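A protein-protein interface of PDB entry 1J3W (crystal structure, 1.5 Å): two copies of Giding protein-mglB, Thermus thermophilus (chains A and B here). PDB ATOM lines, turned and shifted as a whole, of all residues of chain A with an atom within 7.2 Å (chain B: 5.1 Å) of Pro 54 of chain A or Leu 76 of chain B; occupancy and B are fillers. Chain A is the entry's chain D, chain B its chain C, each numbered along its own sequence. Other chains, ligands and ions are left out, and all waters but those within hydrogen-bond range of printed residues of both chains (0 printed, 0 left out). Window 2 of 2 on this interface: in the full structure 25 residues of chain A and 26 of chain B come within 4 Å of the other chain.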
ATOM      1  N   ARG A  30     -15.113   9.276 -12.557  1.00  0.00           N
ATOM      2  CA  ARG A  30     -15.190   9.469 -11.108  1.00  0.00           C
ATOM      3  C   ARG A  30     -15.816   8.307 -10.354  1.00  0.00           C
ATOM      4  O   ARG A  30     -15.262   7.823  -9.371  1.00  0.00           O
ATOM      5  CB  ARG A  30     -16.017  10.707 -10.761  1.00  0.00           C
ATOM      6  CG  ARG A  30     -15.456  12.029 -11.199  1.00  0.00           C
ATOM      7  CD  ARG A  30     -16.238  13.137 -10.515  1.00  0.00           C
ATOM      8  NE  ARG A  30     -15.886  14.447 -11.040  1.00  0.00           N
ATOM      9  CZ  ARG A  30     -16.359  15.591 -10.565  1.00  0.00           C
ATOM     10  NH1 ARG A  30     -17.202  15.593  -9.540  1.00  0.00           N
ATOM     11  NH2 ARG A  30     -16.010  16.731 -11.142  1.00  0.00           N
ATOM     12  N   TYR A  31     -16.997   7.895 -10.802  1.00  0.00           N
ATOM     13  CA  TYR A  31     -17.733   6.824 -10.146  1.00  0.00           C
ATOM     14  C   TYR A  31     -18.183   5.768 -11.140  1.00  0.00           C
ATOM     15  O   TYR A  31     -18.560   6.075 -12.273  1.00  0.00           O
ATOM     16  CB  TYR A  31     -18.960   7.403  -9.433  1.00  0.00           C
ATOM     17  CG  TYR A  31     -18.707   8.740  -8.769  1.00  0.00           C
ATOM     18  CD1 TYR A  31     -17.705   8.887  -7.808  1.00  0.00           C
ATOM     19  CD2 TYR A  31     -19.447   9.866  -9.124  1.00  0.00           C
ATOM     20  CE1 TYR A  31     -17.443  10.121  -7.225  1.00  0.00           C
ATOM     21  CE2 TYR A  31     -19.194  11.108  -8.542  1.00  0.00           C
ATOM     22  CZ  TYR A  31     -18.187  11.226  -7.594  1.00  0.00           C
ATOM     23  OH  TYR A  31     -17.921  12.450  -7.025  1.00  0.00           O
ATOM     24  N   PRO A  51     -14.407  13.752  -5.501  1.00  0.00           N
ATOM     25  CA  PRO A  51     -15.129  14.213  -4.314  1.00  0.00           C
ATOM     26  C   PRO A  51     -16.170  13.164  -3.946  1.00  0.00           C
ATOM     27  O   PRO A  51     -16.435  12.247  -4.729  1.00  0.00           O
ATOM     28  CB  PRO A  51     -15.778  15.514  -4.786  1.00  0.00           C
ATOM     29  CG  PRO A  51     -14.850  15.991  -5.867  1.00  0.00           C
ATOM     30  CD  PRO A  51     -14.555  14.714  -6.608  1.00  0.00           C
ATOM     31  N   LYS A  52     -16.758  13.290  -2.762  1.00  0.00           N
ATOM     32  CA  LYS A  52     -17.782  12.343  -2.343  1.00  0.00           C
ATOM     33  C   LYS A  52     -18.846  12.361  -3.435  1.00  0.00           C
ATOM     34  O   LYS A  52     -19.221  13.423  -3.932  1.00  0.00           O
ATOM     35  CB  LYS A  52     -18.396  12.767  -1.006  1.00  0.00           C
ATOM     36  CG  LYS A  52     -19.133  14.098  -1.050  1.00  0.00           C
ATOM     37  CD  LYS A  52     -19.698  14.480   0.312  1.00  0.00           C
ATOM     38  CE  LYS A  52     -20.740  13.479   0.792  1.00  0.00           C
ATOM     39  NZ  LYS A  52     -21.308  13.863   2.116  1.00  0.00           N
ATOM     40  N   PRO A  53     -19.339  11.181  -3.831  1.00  0.00           N
ATOM     41  CA  PRO A  53     -20.359  11.128  -4.877  1.00  0.00           C
ATOM     42  C   PRO A  53     -21.743  11.505  -4.381  1.00  0.00           C
ATOM     43  O   PRO A  53     -22.001  11.538  -3.176  1.00  0.00           O
ATOM     44  CB  PRO A  53     -20.310   9.670  -5.315  1.00  0.00           C
ATOM     45  CG  PRO A  53     -20.046   8.966  -4.018  1.00  0.00           C
ATOM     46  CD  PRO A  53     -18.946   9.824  -3.412  1.00  0.00           C
ATOM     47  N   PRO A  54     -22.650  11.824  -5.311  1.00  0.00           N
ATOM     48  CA  PRO A  54     -24.005  12.176  -4.889  1.00  0.00           C
ATOM     49  C   PRO A  54     -24.572  10.855  -4.367  1.00  0.00           C
ATOM     50  O   PRO A  54     -23.961   9.803  -4.563  1.00  0.00           O
ATOM     51  CB  PRO A  54     -24.662  12.621  -6.194  1.00  0.00           C
ATOM     52  CG  PRO A  54     -23.962  11.771  -7.224  1.00  0.00           C
ATOM     53  CD  PRO A  54     -22.521  11.866  -6.779  1.00  0.00           C
ATOM     54  N   PRO A  55     -25.728  10.883  -3.688  1.00  0.00           N
ATOM     55  CA  PRO A  55     -26.295   9.629  -3.178  1.00  0.00           C
ATOM     56  C   PRO A  55     -26.331   8.577  -4.287  1.00  0.00           C
ATOM     57  O   PRO A  55     -27.077   8.715  -5.258  1.00  0.00           O
ATOM     58  CB  PRO A  55     -27.686  10.050  -2.718  1.00  0.00           C
ATOM     59  CG  PRO A  55     -27.456  11.453  -2.243  1.00  0.00           C
ATOM     60  CD  PRO A  55     -26.572  12.034  -3.325  1.00  0.00           C
ATOM     61  N   LEU A  56     -25.524   7.530  -4.139  1.00  0.00           N
ATOM     62  CA  LEU A  56     -25.439   6.487  -5.154  1.00  0.00           C
ATOM     63  C   LEU A  56     -26.724   5.716  -5.399  1.00  0.00           C
ATOM     64  O   LEU A  56     -27.004   5.335  -6.532  1.00  0.00           O
ATOM     65  CB  LEU A  56     -24.300   5.519  -4.824  1.00  0.00           C
ATOM     66  CG  LEU A  56     -22.897   6.140  -4.860  1.00  0.00           C
ATOM     67  CD1 LEU A  56     -21.869   5.069  -4.539  1.00  0.00           C
ATOM     68  CD2 LEU A  56     -22.622   6.749  -6.231  1.00  0.00           C
ATOM     69  N   ASP A  57     -27.507   5.476  -4.351  1.00  0.00           N
ATOM     70  CA  ASP A  57     -28.755   4.753  -4.541  1.00  0.00           C
ATOM     71  C   ASP A  57     -29.730   5.606  -5.344  1.00  0.00           C
ATOM     72  O   ASP A  57     -30.476   5.090  -6.175  1.00  0.00           O
ATOM     73  CB  ASP A  57     -29.362   4.361  -3.194  1.00  0.00           C
ATOM     74  CG  ASP A  57     -28.481   3.398  -2.426  1.00  0.00           C
ATOM     75  OD1 ASP A  57     -27.956   2.451  -3.051  1.00  0.00           O
ATOM     76  OD2 ASP A  57     -28.316   3.583  -1.201  1.00  0.00           O
ATOM     77  N   THR A  58     -29.716   6.913  -5.107  1.00  0.00           N
ATOM     78  CA  THR A  58     -30.595   7.812  -5.851  1.00  0.00           C
ATOM     79  C   THR A  58     -30.128   7.867  -7.305  1.00  0.00           C
ATOM     80  O   THR A  58     -30.943   7.855  -8.231  1.00  0.00           O
ATOM     81  CB  THR A  58     -30.584   9.224  -5.250  1.00  0.00           C
ATOM     82  OG1 THR A  58     -31.006   9.157  -3.882  1.00  0.00           O
ATOM     83  CG2 THR A  58     -31.534  10.139  -6.016  1.00  0.00           C
ATOM     84  N   LEU A  59     -28.813   7.923  -7.506  1.00  0.00           N
ATOM     85  CA  LEU A  59     -28.266   7.947  -8.857  1.00  0.00           C
ATOM     86  C   LEU A  59     -28.714   6.703  -9.618  1.00  0.00           C
ATOM     87  O   LEU A  59     -29.204   6.792 -10.748  1.00  0.00           O
ATOM     88  CB  LEU A  59     -26.730   7.993  -8.813  1.00  0.00           C
ATOM     89  CG  LEU A  59     -25.993   7.822 -10.146  1.00  0.00           C
ATOM     90  CD1 LEU A  59     -26.383   8.931 -11.101  1.00  0.00           C
ATOM     91  CD2 LEU A  59     -24.487   7.828  -9.898  1.00  0.00           C
ATOM     92  N   ALA A  60     -28.540   5.541  -8.994  1.00  0.00           N
ATOM     93  CA  ALA A  60     -28.924   4.275  -9.605  1.00  0.00           C
ATOM     94  C   ALA A  60     -30.420   4.253  -9.908  1.00  0.00           C
ATOM     95  O   ALA A  60     -30.840   3.779 -10.960  1.00  0.00           O
ATOM     96  CB  ALA A  60     -28.563   3.115  -8.681  1.00  0.00           C
ATOM     97  N   LEU A  62     -32.426   6.808 -10.512  1.00  0.00           N
ATOM     98  CA  LEU A  62     -32.686   7.684 -11.648  1.00  0.00           C
ATOM     99  C   LEU A  62     -32.229   7.057 -12.963  1.00  0.00           C
ATOM    100  O   LEU A  62     -32.890   7.204 -13.986  1.00  0.00           O
ATOM    101  CB  LEU A  62     -32.005   9.041 -11.443  1.00  0.00           C
ATOM    102  CG  LEU A  62     -32.557   9.875 -10.282  1.00  0.00           C
ATOM    103  CD1 LEU A  62     -31.766  11.165 -10.147  1.00  0.00           C
ATOM    104  CD2 LEU A  62     -34.035  10.175 -10.533  1.00  0.00           C
ATOM    105  N   MET A  92     -20.274  17.847 -16.011  1.00  0.00           N
ATOM    106  CA  MET A  92     -20.486  16.440 -15.697  1.00  0.00           C
ATOM    107  C   MET A  92     -21.128  15.647 -16.825  1.00  0.00           C
ATOM    108  O   MET A  92     -21.934  16.173 -17.593  1.00  0.00           O
ATOM    109  CB  MET A  92     -21.350  16.312 -14.442  1.00  0.00           C
ATOM    110  CG  MET A  92     -20.725  16.893 -13.187  1.00  0.00           C
ATOM    111  SD  MET A  92     -19.185  16.063 -12.746  1.00  0.00           S
ATOM    112  CE  MET A  92     -19.805  14.635 -11.868  1.00  0.00           C
ATOM    113  N   VAL A 108     -19.817   7.823 -14.186  1.00  0.00           N
ATOM    114  CA  VAL A 108     -20.038   9.253 -14.024  1.00  0.00           C
ATOM    115  C   VAL A 108     -18.666   9.875 -14.224  1.00  0.00           C
ATOM    116  O   VAL A 108     -17.689   9.431 -13.616  1.00  0.00           O
ATOM    117  CB  VAL A 108     -20.548   9.590 -12.611  1.00  0.00           C
ATOM    118  CG1 VAL A 108     -20.719  11.090 -12.464  1.00  0.00           C
ATOM    119  CG2 VAL A 108     -21.874   8.876 -12.355  1.00  0.00           C
ATOM    120  N   GLN B  71     -33.755  15.637 -16.483  1.00  0.00           N
ATOM    121  CA  GLN B  71     -33.310  16.761 -15.669  1.00  0.00           C
ATOM    122  C   GLN B  71     -33.017  16.389 -14.222  1.00  0.00           C
ATOM    123  O   GLN B  71     -32.146  16.992 -13.592  1.00  0.00           O
ATOM    124  CB  GLN B  71     -34.325  17.903 -15.747  1.00  0.00           C
ATOM    125  CG  GLN B  71     -34.325  18.558 -17.119  1.00  0.00           C
ATOM    126  CD  GLN B  71     -35.130  19.836 -17.178  1.00  0.00           C
ATOM    127  OE1 GLN B  71     -35.060  20.670 -16.275  1.00  0.00           O
ATOM    128  NE2 GLN B  71     -35.887  20.007 -18.256  1.00  0.00           N
ATOM    129  N   ALA B  72     -33.729  15.397 -13.697  1.00  0.00           N
ATOM    130  CA  ALA B  72     -33.504  14.955 -12.322  1.00  0.00           C
ATOM    131  C   ALA B  72     -32.073  14.434 -12.215  1.00  0.00           C
ATOM    132  O   ALA B  72     -31.348  14.780 -11.275  1.00  0.00           O
ATOM    133  CB  ALA B  72     -34.495  13.861 -11.948  1.00  0.00           C
ATOM    134  N   LEU B  73     -31.679  13.599 -13.177  1.00  0.00           N
ATOM    135  CA  LEU B  73     -30.325  13.040 -13.217  1.00  0.00           C
ATOM    136  C   LEU B  73     -29.306  14.164 -13.355  1.00  0.00           C
ATOM    137  O   LEU B  73     -28.284  14.179 -12.667  1.00  0.00           O
ATOM    138  CB  LEU B  73     -30.174  12.083 -14.404  1.00  0.00           C
ATOM    139  CG  LEU B  73     -30.425  10.589 -14.189  1.00  0.00           C
ATOM    140  CD1 LEU B  73     -30.478   9.881 -15.537  1.00  0.00           C
ATOM    141  CD2 LEU B  73     -29.324  10.001 -13.315  1.00  0.00           C
ATOM    142  N   ALA B  74     -29.586  15.104 -14.251  1.00  0.00           N
ATOM    143  CA  ALA B  74     -28.686  16.228 -14.467  1.00  0.00           C
ATOM    144  C   ALA B  74     -28.472  16.990 -13.165  1.00  0.00           C
ATOM    145  O   ALA B  74     -27.336  17.268 -12.774  1.00  0.00           O
ATOM    146  CB  ALA B  74     -29.259  17.158 -15.526  1.00  0.00           C
ATOM    147  N   LYS B  75     -29.568  17.319 -12.489  1.00  0.00           N
ATOM    148  CA  LYS B  75     -29.489  18.067 -11.240  1.00  0.00           C
ATOM    149  C   LYS B  75     -28.744  17.326 -10.136  1.00  0.00           C
ATOM    150  O   LYS B  75     -28.046  17.949  -9.332  1.00  0.00           O
ATOM    151  CB  LYS B  75     -30.895  18.459 -10.781  1.00  0.00           C
ATOM    152  CG  LYS B  75     -31.527  19.510 -11.677  1.00  0.00           C
ATOM    153  CD  LYS B  75     -32.898  19.936 -11.189  1.00  0.00           C
ATOM    154  CE  LYS B  75     -33.408  21.122 -11.993  1.00  0.00           C
ATOM    155  NZ  LYS B  75     -33.477  20.820 -13.450  1.00  0.00           N
ATOM    156  N   LEU B  76     -28.875  16.005 -10.099  1.00  0.00           N
ATOM    157  CA  LEU B  76     -28.182  15.218  -9.085  1.00  0.00           C
ATOM    158  C   LEU B  76     -26.680  15.366  -9.301  1.00  0.00           C
ATOM    159  O   LEU B  76     -25.898  15.342  -8.350  1.00  0.00           O
ATOM    160  CB  LEU B  76     -28.562  13.739  -9.182  1.00  0.00           C
ATOM    161  CG  LEU B  76     -28.042  12.884  -8.022  1.00  0.00           C
ATOM    162  CD1 LEU B  76     -28.756  13.304  -6.749  1.00  0.00           C
ATOM    163  CD2 LEU B  76     -28.270  11.409  -8.290  1.00  0.00           C
ATOM    164  N   LEU B  77     -26.286  15.528 -10.561  1.00  0.00           N
ATOM    165  CA  LEU B  77     -24.877  15.675 -10.912  1.00  0.00           C
ATOM    166  C   LEU B  77     -24.419  17.134 -10.919  1.00  0.00           C
ATOM    167  O   LEU B  77     -23.310  17.439 -11.362  1.00  0.00           O
ATOM    168  CB  LEU B  77     -24.609  15.031 -12.276  1.00  0.00           C
ATOM    169  CG  LEU B  77     -24.876  13.524 -12.348  1.00  0.00           C
ATOM    170  CD1 LEU B  77     -24.567  13.003 -13.746  1.00  0.00           C
ATOM    171  CD2 LEU B  77     -24.024  12.801 -11.312  1.00  0.00           C
ATOM    172  N   GLY B  78     -25.275  18.030 -10.433  1.00  0.00           N
ATOM    173  CA  GLY B  78     -24.922  19.440 -10.366  1.00  0.00           C
ATOM    174  C   GLY B  78     -25.174  20.269 -11.615  1.00  0.00           C
ATOM    175  O   GLY B  78     -24.740  21.421 -11.698  1.00  0.00           O
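NH2 of Arg 30 of chain A lies close to SD of Met 92 of chain A (3.6 Å).
O of Val 108 of chain A is in hydrogen-bond range of N of Arg 30 of chain A, at 2.8 Å.
The backbone carbonyl oxygen (O) of Tyr 31 of chain A is in hydrogen-bond range of the backbone NH (N) of Val 108 of chain A, at 2.9 Å.
Printed residues of chain A that touch a printed residue of chain B: Pro 54, Leu 59, Leu 62, Met 92 and Val 108.
Among the printed residues, no Asp or Glu carboxylate lies within 4 Å of a Lys or Arg side-chain nitrogen of the other chain.
No position is printed for both chains.
Of the 8 pairs that touch across the chains among the printed residues, none has its exchanged pair printed and touching as well.
Pro 54 of chain A touches Leu 76 of chain B (CB to O, 3.7 Å).
CD1 of Leu 59 of chain A touches CD2 of Leu 73 of chain B (3.8 Å).
Leu 76 of chain B touches Leu 59 of chain A.
Ala 72 of chain B touches Leu 62 of chain A (O to CD1, 3.8 Å).
Leu 73 of chain B touches Leu 62 of chain A.
CD1 of Leu 62 of chain A touches CD2 of Leu 76 of chain B, at 3.97 Å.
Met 92 of chain A touches Leu 77 of chain B (CG to O, 3.2 Å).
Val 108 of chain A touches Leu 77 of chain B.
Ala 60 of chain A touches none of the printed residues of chain B.
Of the printed residues of chain B, Leu 62 of chain A touches Ala 72 (3.8 Å), Leu 73 (3.4 Å) and Leu 76 (3.97 Å).
Printed residues of chain B within 4 Å of Val 108 of chain A: Leu 77 (3.9 Å).
Ala 74 of chain B touches none of the printed residues of chain A.
Of chain A, only Pro 54, Leu 59 and Leu 62 come within 4 Å of Leu 76 of chain B.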
